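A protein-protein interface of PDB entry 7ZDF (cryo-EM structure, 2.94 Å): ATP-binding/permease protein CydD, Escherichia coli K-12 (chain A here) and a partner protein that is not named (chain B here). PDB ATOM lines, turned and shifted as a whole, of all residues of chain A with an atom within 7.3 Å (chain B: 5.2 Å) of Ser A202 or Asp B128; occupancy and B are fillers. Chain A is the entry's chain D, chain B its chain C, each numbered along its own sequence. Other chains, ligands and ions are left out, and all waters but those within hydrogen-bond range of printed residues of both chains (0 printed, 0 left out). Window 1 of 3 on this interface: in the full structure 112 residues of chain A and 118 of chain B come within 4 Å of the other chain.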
ATOM      1  N   LEU A 196      35.024 -20.119 -17.025  1.00  0.00           N
ATOM      2  CA  LEU A 196      34.638 -21.460 -17.448  1.00  0.00           C
ATOM      3  C   LEU A 196      34.260 -22.322 -16.251  1.00  0.00           C
ATOM      4  O   LEU A 196      33.309 -23.108 -16.318  1.00  0.00           O
ATOM      5  CB  LEU A 196      35.772 -22.108 -18.240  1.00  0.00           C
ATOM      6  CG  LEU A 196      35.995 -21.597 -19.663  1.00  0.00           C
ATOM      7  CD1 LEU A 196      37.341 -22.057 -20.191  1.00  0.00           C
ATOM      8  CD2 LEU A 196      34.875 -22.059 -20.576  1.00  0.00           C
ATOM      9  N   ALA A 197      34.998 -22.190 -15.148  1.00  0.00           N
ATOM     10  CA  ALA A 197      34.660 -22.931 -13.937  1.00  0.00           C
ATOM     11  C   ALA A 197      33.327 -22.470 -13.360  1.00  0.00           C
ATOM     12  O   ALA A 197      32.546 -23.290 -12.868  1.00  0.00           O
ATOM     13  CB  ALA A 197      35.775 -22.783 -12.905  1.00  0.00           C
ATOM     14  N   LEU A 198      33.054 -21.164 -13.404  1.00  0.00           N
ATOM     15  CA  LEU A 198      31.772 -20.664 -12.917  1.00  0.00           C
ATOM     16  C   LEU A 198      30.619 -21.167 -13.776  1.00  0.00           C
ATOM     17  O   LEU A 198      29.555 -21.517 -13.253  1.00  0.00           O
ATOM     18  CB  LEU A 198      31.785 -19.136 -12.877  1.00  0.00           C
ATOM     19  CG  LEU A 198      30.488 -18.460 -12.427  1.00  0.00           C
ATOM     20  CD1 LEU A 198      30.220 -18.714 -10.954  1.00  0.00           C
ATOM     21  CD2 LEU A 198      30.532 -16.970 -12.716  1.00  0.00           C
ATOM     22  N   ALA A 199      30.807 -21.203 -15.096  1.00  0.00           N
ATOM     23  CA  ALA A 199      29.783 -21.763 -15.970  1.00  0.00           C
ATOM     24  C   ALA A 199      29.670 -23.270 -15.801  1.00  0.00           C
ATOM     25  O   ALA A 199      28.581 -23.832 -15.958  1.00  0.00           O
ATOM     26  CB  ALA A 199      30.085 -21.414 -17.426  1.00  0.00           C
ATOM     27  N   ARG A 200      30.781 -23.941 -15.490  1.00  0.00           N
ATOM     28  CA  ARG A 200      30.730 -25.373 -15.222  1.00  0.00           C
ATOM     29  C   ARG A 200      30.131 -25.649 -13.849  1.00  0.00           C
ATOM     30  O   ARG A 200      29.408 -26.635 -13.668  1.00  0.00           O
ATOM     31  CB  ARG A 200      32.131 -25.968 -15.343  1.00  0.00           C
ATOM     32  CG  ARG A 200      32.317 -27.319 -14.684  1.00  0.00           C
ATOM     33  CD  ARG A 200      33.785 -27.688 -14.659  1.00  0.00           C
ATOM     34  NE  ARG A 200      34.483 -27.166 -15.831  1.00  0.00           N
ATOM     35  CZ  ARG A 200      35.670 -26.573 -15.790  1.00  0.00           C
ATOM     36  NH1 ARG A 200      36.229 -26.129 -16.907  1.00  0.00           N
ATOM     37  NH2 ARG A 200      36.300 -26.423 -14.634  1.00  0.00           N
ATOM     38  N   LEU A 201      30.414 -24.786 -12.872  1.00  0.00           N
ATOM     39  CA  LEU A 201      29.751 -24.893 -11.578  1.00  0.00           C
ATOM     40  C   LEU A 201      28.258 -24.629 -11.700  1.00  0.00           C
ATOM     41  O   LEU A 201      27.467 -25.168 -10.919  1.00  0.00           O
ATOM     42  CB  LEU A 201      30.389 -23.923 -10.583  1.00  0.00           C
ATOM     43  CG  LEU A 201      29.802 -23.850  -9.175  1.00  0.00           C
ATOM     44  CD1 LEU A 201      30.283 -25.021  -8.344  1.00  0.00           C
ATOM     45  CD2 LEU A 201      30.169 -22.537  -8.515  1.00  0.00           C
ATOM     46  N   SER A 202      27.853 -23.813 -12.674  1.00  0.00           N
ATOM     47  CA  SER A 202      26.436 -23.590 -12.925  1.00  0.00           C
ATOM     48  C   SER A 202      25.781 -24.790 -13.589  1.00  0.00           C
ATOM     49  O   SER A 202      24.561 -24.949 -13.485  1.00  0.00           O
ATOM     50  CB  SER A 202      26.247 -22.343 -13.789  1.00  0.00           C
ATOM     51  OG  SER A 202      24.875 -22.051 -13.976  1.00  0.00           O
ATOM     52  N   GLY A 203      26.561 -25.633 -14.272  1.00  0.00           N
ATOM     53  CA  GLY A 203      26.037 -26.881 -14.793  1.00  0.00           C
ATOM     54  C   GLY A 203      26.039 -28.011 -13.792  1.00  0.00           C
ATOM     55  O   GLY A 203      25.328 -29.000 -13.987  1.00  0.00           O
ATOM     56  N   HIS A 204      26.834 -27.886 -12.729  1.00  0.00           N
ATOM     57  CA  HIS A 204      26.761 -28.836 -11.625  1.00  0.00           C
ATOM     58  C   HIS A 204      25.511 -28.596 -10.790  1.00  0.00           C
ATOM     59  O   HIS A 204      24.935 -29.540 -10.238  1.00  0.00           O
ATOM     60  CB  HIS A 204      28.032 -28.731 -10.779  1.00  0.00           C
ATOM     61  CG  HIS A 204      27.901 -29.287  -9.396  1.00  0.00           C
ATOM     62  ND1 HIS A 204      28.375 -30.534  -9.049  1.00  0.00           N
ATOM     63  CD2 HIS A 204      27.387 -28.753  -8.263  1.00  0.00           C
ATOM     64  CE1 HIS A 204      28.139 -30.753  -7.769  1.00  0.00           C
ATOM     65  NE2 HIS A 204      27.539 -29.688  -7.268  1.00  0.00           N
ATOM     66  N   PHE A 205      25.076 -27.340 -10.688  1.00  0.00           N
ATOM     67  CA  PHE A 205      23.816 -27.044 -10.015  1.00  0.00           C
ATOM     68  C   PHE A 205      22.627 -27.514 -10.842  1.00  0.00           C
ATOM     69  O   PHE A 205      21.671 -28.076 -10.299  1.00  0.00           O
ATOM     70  CB  PHE A 205      23.712 -25.546  -9.732  1.00  0.00           C
ATOM     71  CG  PHE A 205      22.474 -25.154  -8.978  1.00  0.00           C
ATOM     72  CD1 PHE A 205      22.171 -25.741  -7.763  1.00  0.00           C
ATOM     73  CD2 PHE A 205      21.613 -24.196  -9.484  1.00  0.00           C
ATOM     74  CE1 PHE A 205      21.036 -25.381  -7.070  1.00  0.00           C
ATOM     75  CE2 PHE A 205      20.477 -23.834  -8.794  1.00  0.00           C
ATOM     76  CZ  PHE A 205      20.189 -24.426  -7.587  1.00  0.00           C
ATOM     77  N   LEU A 206      22.666 -27.284 -12.156  1.00  0.00           N
ATOM     78  CA  LEU A 206      21.585 -27.740 -13.022  1.00  0.00           C
ATOM     79  C   LEU A 206      21.529 -29.259 -13.090  1.00  0.00           C
ATOM     80  O   LEU A 206      20.440 -29.832 -13.206  1.00  0.00           O
ATOM     81  CB  LEU A 206      21.750 -27.149 -14.420  1.00  0.00           C
ATOM     82  CG  LEU A 206      20.747 -27.601 -15.480  1.00  0.00           C
ATOM     83  CD1 LEU A 206      19.358 -27.087 -15.156  1.00  0.00           C
ATOM     84  CD2 LEU A 206      21.183 -27.137 -16.853  1.00  0.00           C
ATOM     85  N   ASP A 207      22.683 -29.923 -13.022  1.00  0.00           N
ATOM     86  CA  ASP A 207      22.699 -31.380 -12.990  1.00  0.00           C
ATOM     87  C   ASP A 207      22.002 -31.911 -11.744  1.00  0.00           C
ATOM     88  O   ASP A 207      21.268 -32.902 -11.808  1.00  0.00           O
ATOM     89  CB  ASP A 207      24.137 -31.886 -13.057  1.00  0.00           C
ATOM     90  CG  ASP A 207      24.218 -33.391 -13.142  1.00  0.00           C
ATOM     91  OD1 ASP A 207      23.545 -33.975 -14.015  1.00  0.00           O
ATOM     92  OD2 ASP A 207      24.957 -33.992 -12.334  1.00  0.00           O
ATOM     93  N   LEU B  92      25.847 -16.612  -3.559  1.00  0.00           N
ATOM     94  CA  LEU B  92      25.516 -17.544  -4.630  1.00  0.00           C
ATOM     95  C   LEU B  92      25.478 -18.974  -4.115  1.00  0.00           C
ATOM     96  O   LEU B  92      24.578 -19.743  -4.462  1.00  0.00           O
ATOM     97  CB  LEU B  92      26.520 -17.415  -5.774  1.00  0.00           C
ATOM     98  CG  LEU B  92      26.291 -18.329  -6.978  1.00  0.00           C
ATOM     99  CD1 LEU B  92      25.021 -17.945  -7.719  1.00  0.00           C
ATOM    100  CD2 LEU B  92      27.488 -18.283  -7.902  1.00  0.00           C
ATOM    101  N   ARG B  96      22.054 -21.183  -3.943  1.00  0.00           N
ATOM    102  CA  ARG B  96      21.935 -22.511  -4.532  1.00  0.00           C
ATOM    103  C   ARG B  96      21.490 -23.537  -3.498  1.00  0.00           C
ATOM    104  O   ARG B  96      20.687 -24.426  -3.803  1.00  0.00           O
ATOM    105  CB  ARG B  96      23.261 -22.933  -5.162  1.00  0.00           C
ATOM    106  CG  ARG B  96      23.713 -22.112  -6.362  1.00  0.00           C
ATOM    107  CD  ARG B  96      24.678 -22.933  -7.206  1.00  0.00           C
ATOM    108  NE  ARG B  96      25.537 -22.140  -8.081  1.00  0.00           N
ATOM    109  CZ  ARG B  96      25.162 -21.640  -9.254  1.00  0.00           C
ATOM    110  NH1 ARG B  96      23.934 -21.835  -9.704  1.00  0.00           N
ATOM    111  NH2 ARG B  96      26.022 -20.941  -9.979  1.00  0.00           N
ATOM    112  N   VAL B 124      17.982 -21.851 -12.901  1.00  0.00           N
ATOM    113  CA  VAL B 124      19.393 -21.584 -12.642  1.00  0.00           C
ATOM    114  C   VAL B 124      19.752 -20.160 -13.046  1.00  0.00           C
ATOM    115  O   VAL B 124      20.551 -19.494 -12.379  1.00  0.00           O
ATOM    116  CB  VAL B 124      20.268 -22.623 -13.366  1.00  0.00           C
ATOM    117  CG1 VAL B 124      21.736 -22.269 -13.243  1.00  0.00           C
ATOM    118  CG2 VAL B 124      20.010 -24.009 -12.808  1.00  0.00           C
ATOM    119  N   ALA B 125      19.165 -19.668 -14.138  1.00  0.00           N
ATOM    120  CA  ALA B 125      19.427 -18.297 -14.558  1.00  0.00           C
ATOM    121  C   ALA B 125      18.844 -17.285 -13.581  1.00  0.00           C
ATOM    122  O   ALA B 125      19.379 -16.180 -13.447  1.00  0.00           O
ATOM    123  CB  ALA B 125      18.869 -18.061 -15.960  1.00  0.00           C
ATOM    124  N   ASP B 126      17.753 -17.636 -12.899  1.00  0.00           N
ATOM    125  CA  ASP B 126      17.164 -16.719 -11.930  1.00  0.00           C
ATOM    126  C   ASP B 126      17.976 -16.674 -10.644  1.00  0.00           C
ATOM    127  O   ASP B 126      18.043 -15.633  -9.983  1.00  0.00           O
ATOM    128  CB  ASP B 126      15.721 -17.121 -11.637  1.00  0.00           C
ATOM    129  CG  ASP B 126      14.787 -16.795 -12.776  1.00  0.00           C
ATOM    130  OD1 ASP B 126      13.608 -17.194 -12.713  1.00  0.00           O
ATOM    131  OD2 ASP B 126      15.233 -16.138 -13.739  1.00  0.00           O
ATOM    132  N   VAL B 127      18.587 -17.796 -10.264  1.00  0.00           N
ATOM    133  CA  VAL B 127      19.440 -17.805  -9.080  1.00  0.00           C
ATOM    134  C   VAL B 127      20.679 -16.953  -9.321  1.00  0.00           C
ATOM    135  O   VAL B 127      21.161 -16.259  -8.418  1.00  0.00           O
ATOM    136  CB  VAL B 127      19.796 -19.253  -8.693  1.00  0.00           C
ATOM    137  CG1 VAL B 127      20.989 -19.289  -7.754  1.00  0.00           C
ATOM    138  CG2 VAL B 127      18.601 -19.930  -8.054  1.00  0.00           C
ATOM    139  N   ASP B 128      21.204 -16.981 -10.546  1.00  0.00           N
ATOM    140  CA  ASP B 128      22.320 -16.109 -10.897  1.00  0.00           C
ATOM    141  C   ASP B 128      21.919 -14.641 -10.825  1.00  0.00           C
ATOM    142  O   ASP B 128      22.696 -13.802 -10.357  1.00  0.00           O
ATOM    143  CB  ASP B 128      22.833 -16.456 -12.293  1.00  0.00           C
ATOM    144  CG  ASP B 128      23.819 -17.604 -12.283  1.00  0.00           C
ATOM    145  OD1 ASP B 128      24.855 -17.492 -11.596  1.00  0.00           O
ATOM    146  OD2 ASP B 128      23.562 -18.618 -12.964  1.00  0.00           O
ATOM    147  N   THR B 129      20.712 -14.309 -11.290  1.00  0.00           N
ATOM    148  CA  THR B 129      20.271 -12.918 -11.281  1.00  0.00           C
ATOM    149  C   THR B 129      20.009 -12.418  -9.867  1.00  0.00           C
ATOM    150  O   THR B 129      20.240 -11.239  -9.577  1.00  0.00           O
ATOM    151  CB  THR B 129      19.021 -12.759 -12.145  1.00  0.00           C
ATOM    152  OG1 THR B 129      19.276 -13.284 -13.452  1.00  0.00           O
ATOM    153  CG2 THR B 129      18.637 -11.296 -12.272  1.00  0.00           C
ATOM    154  N   LEU B 130      19.538 -13.289  -8.973  1.00  0.00           N
ATOM    155  CA  LEU B 130      19.407 -12.899  -7.573  1.00  0.00           C
ATOM    156  C   LEU B 130      20.768 -12.682  -6.933  1.00  0.00           C
ATOM    157  O   LEU B 130      20.884 -11.940  -5.951  1.00  0.00           O
ATOM    158  CB  LEU B 130      18.620 -13.956  -6.801  1.00  0.00           C
ATOM    159  CG  LEU B 130      17.152 -14.127  -7.188  1.00  0.00           C
ATOM    160  CD1 LEU B 130      16.506 -15.218  -6.359  1.00  0.00           C
ATOM    161  CD2 LEU B 130      16.410 -12.817  -7.018  1.00  0.00           C
ATOM    162  N   ASP B 131      21.808 -13.322  -7.471  1.00  0.00           N
ATOM    163  CA  ASP B 131      23.162 -13.118  -6.977  1.00  0.00           C
ATOM    164  C   ASP B 131      23.716 -11.756  -7.374  1.00  0.00           C
ATOM    165  O   ASP B 131      24.664 -11.276  -6.746  1.00  0.00           O
ATOM    166  CB  ASP B 131      24.066 -14.237  -7.494  1.00  0.00           C
ATOM    167  CG  ASP B 131      25.475 -14.147  -6.959  1.00  0.00           C
ATOM    168  OD1 ASP B 131      26.424 -14.362  -7.740  1.00  0.00           O
ATOM    169  OD2 ASP B 131      25.633 -13.861  -5.759  1.00  0.00           O
ATOM    170  N   HIS B 132      23.135 -11.118  -8.388  1.00  0.00           N
ATOM    171  CA  HIS B 132      23.573  -9.815  -8.864  1.00  0.00           C
ATOM    172  C   HIS B 132      22.972  -8.660  -8.079  1.00  0.00           C
ATOM    173  O   HIS B 132      23.282  -7.504  -8.376  1.00  0.00           O
ATOM    174  CB  HIS B 132      23.220  -9.647 -10.343  1.00  0.00           C
ATOM    175  CG  HIS B 132      23.825 -10.686 -11.231  1.00  0.00           C
ATOM    176  ND1 HIS B 132      23.418 -10.876 -12.534  1.00  0.00           N
ATOM    177  CD2 HIS B 132      24.807 -11.590 -11.007  1.00  0.00           C
ATOM    178  CE1 HIS B 132      24.123 -11.855 -13.073  1.00  0.00           C
ATOM    179  NE2 HIS B 132      24.972 -12.305 -12.168  1.00  0.00           N
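The side-chain carboxylate (OD1) of Asp B128 lies within salt-bridge range of the guanidinium group (NH2) of Arg B96, at 3.98 Å. O of Asp B128 sits close to NE2 of His B132, 3.3 Å away.
Among the printed residues, pairs that only touch across the chains: Ser A202 with Arg B96, Ser A202 with Val B124, Ser A202 with Asp B128, Phe A205 with Arg B96, Phe A205 with Val B124 and Leu A206 with Val B124.
Of the 11 printed residues of chain B, 3 touch a printed residue of chain A. Printed residues of chain B that touch a printed residue of chain A: Arg B96, Val B124 and Asp B128. Along chain B the printed residues that touch a printed residue of chain A span positions 96 to 128. Hydrophobic or aromatic side chains of chain A that line the printed part of chain B: Phe A205 and Leu A206. Along chain A the printed residues that touch a printed residue of chain B span positions 202 to 206. Among the printed residues, 6 pairs touch across the chains.
Of the printed residues of chain B, Ser A202 touches Arg B96 (3.98 Å), Val B124 (3.2 Å) and Asp B128 (3.8 Å). Of chain A, only Ser A202 comes within 4 Å of Asp B128. Printed residues of chain B within 4 Å of Phe A205: Arg B96 (3.3 Å) and Val B124 (3.7 Å). Printed residues of chain A within 4 Å of Arg B96: Ser A202 and Phe A205. The nearest printed residue of chain A that does not touch Arg B96 is Leu A201 (4.5 Å).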
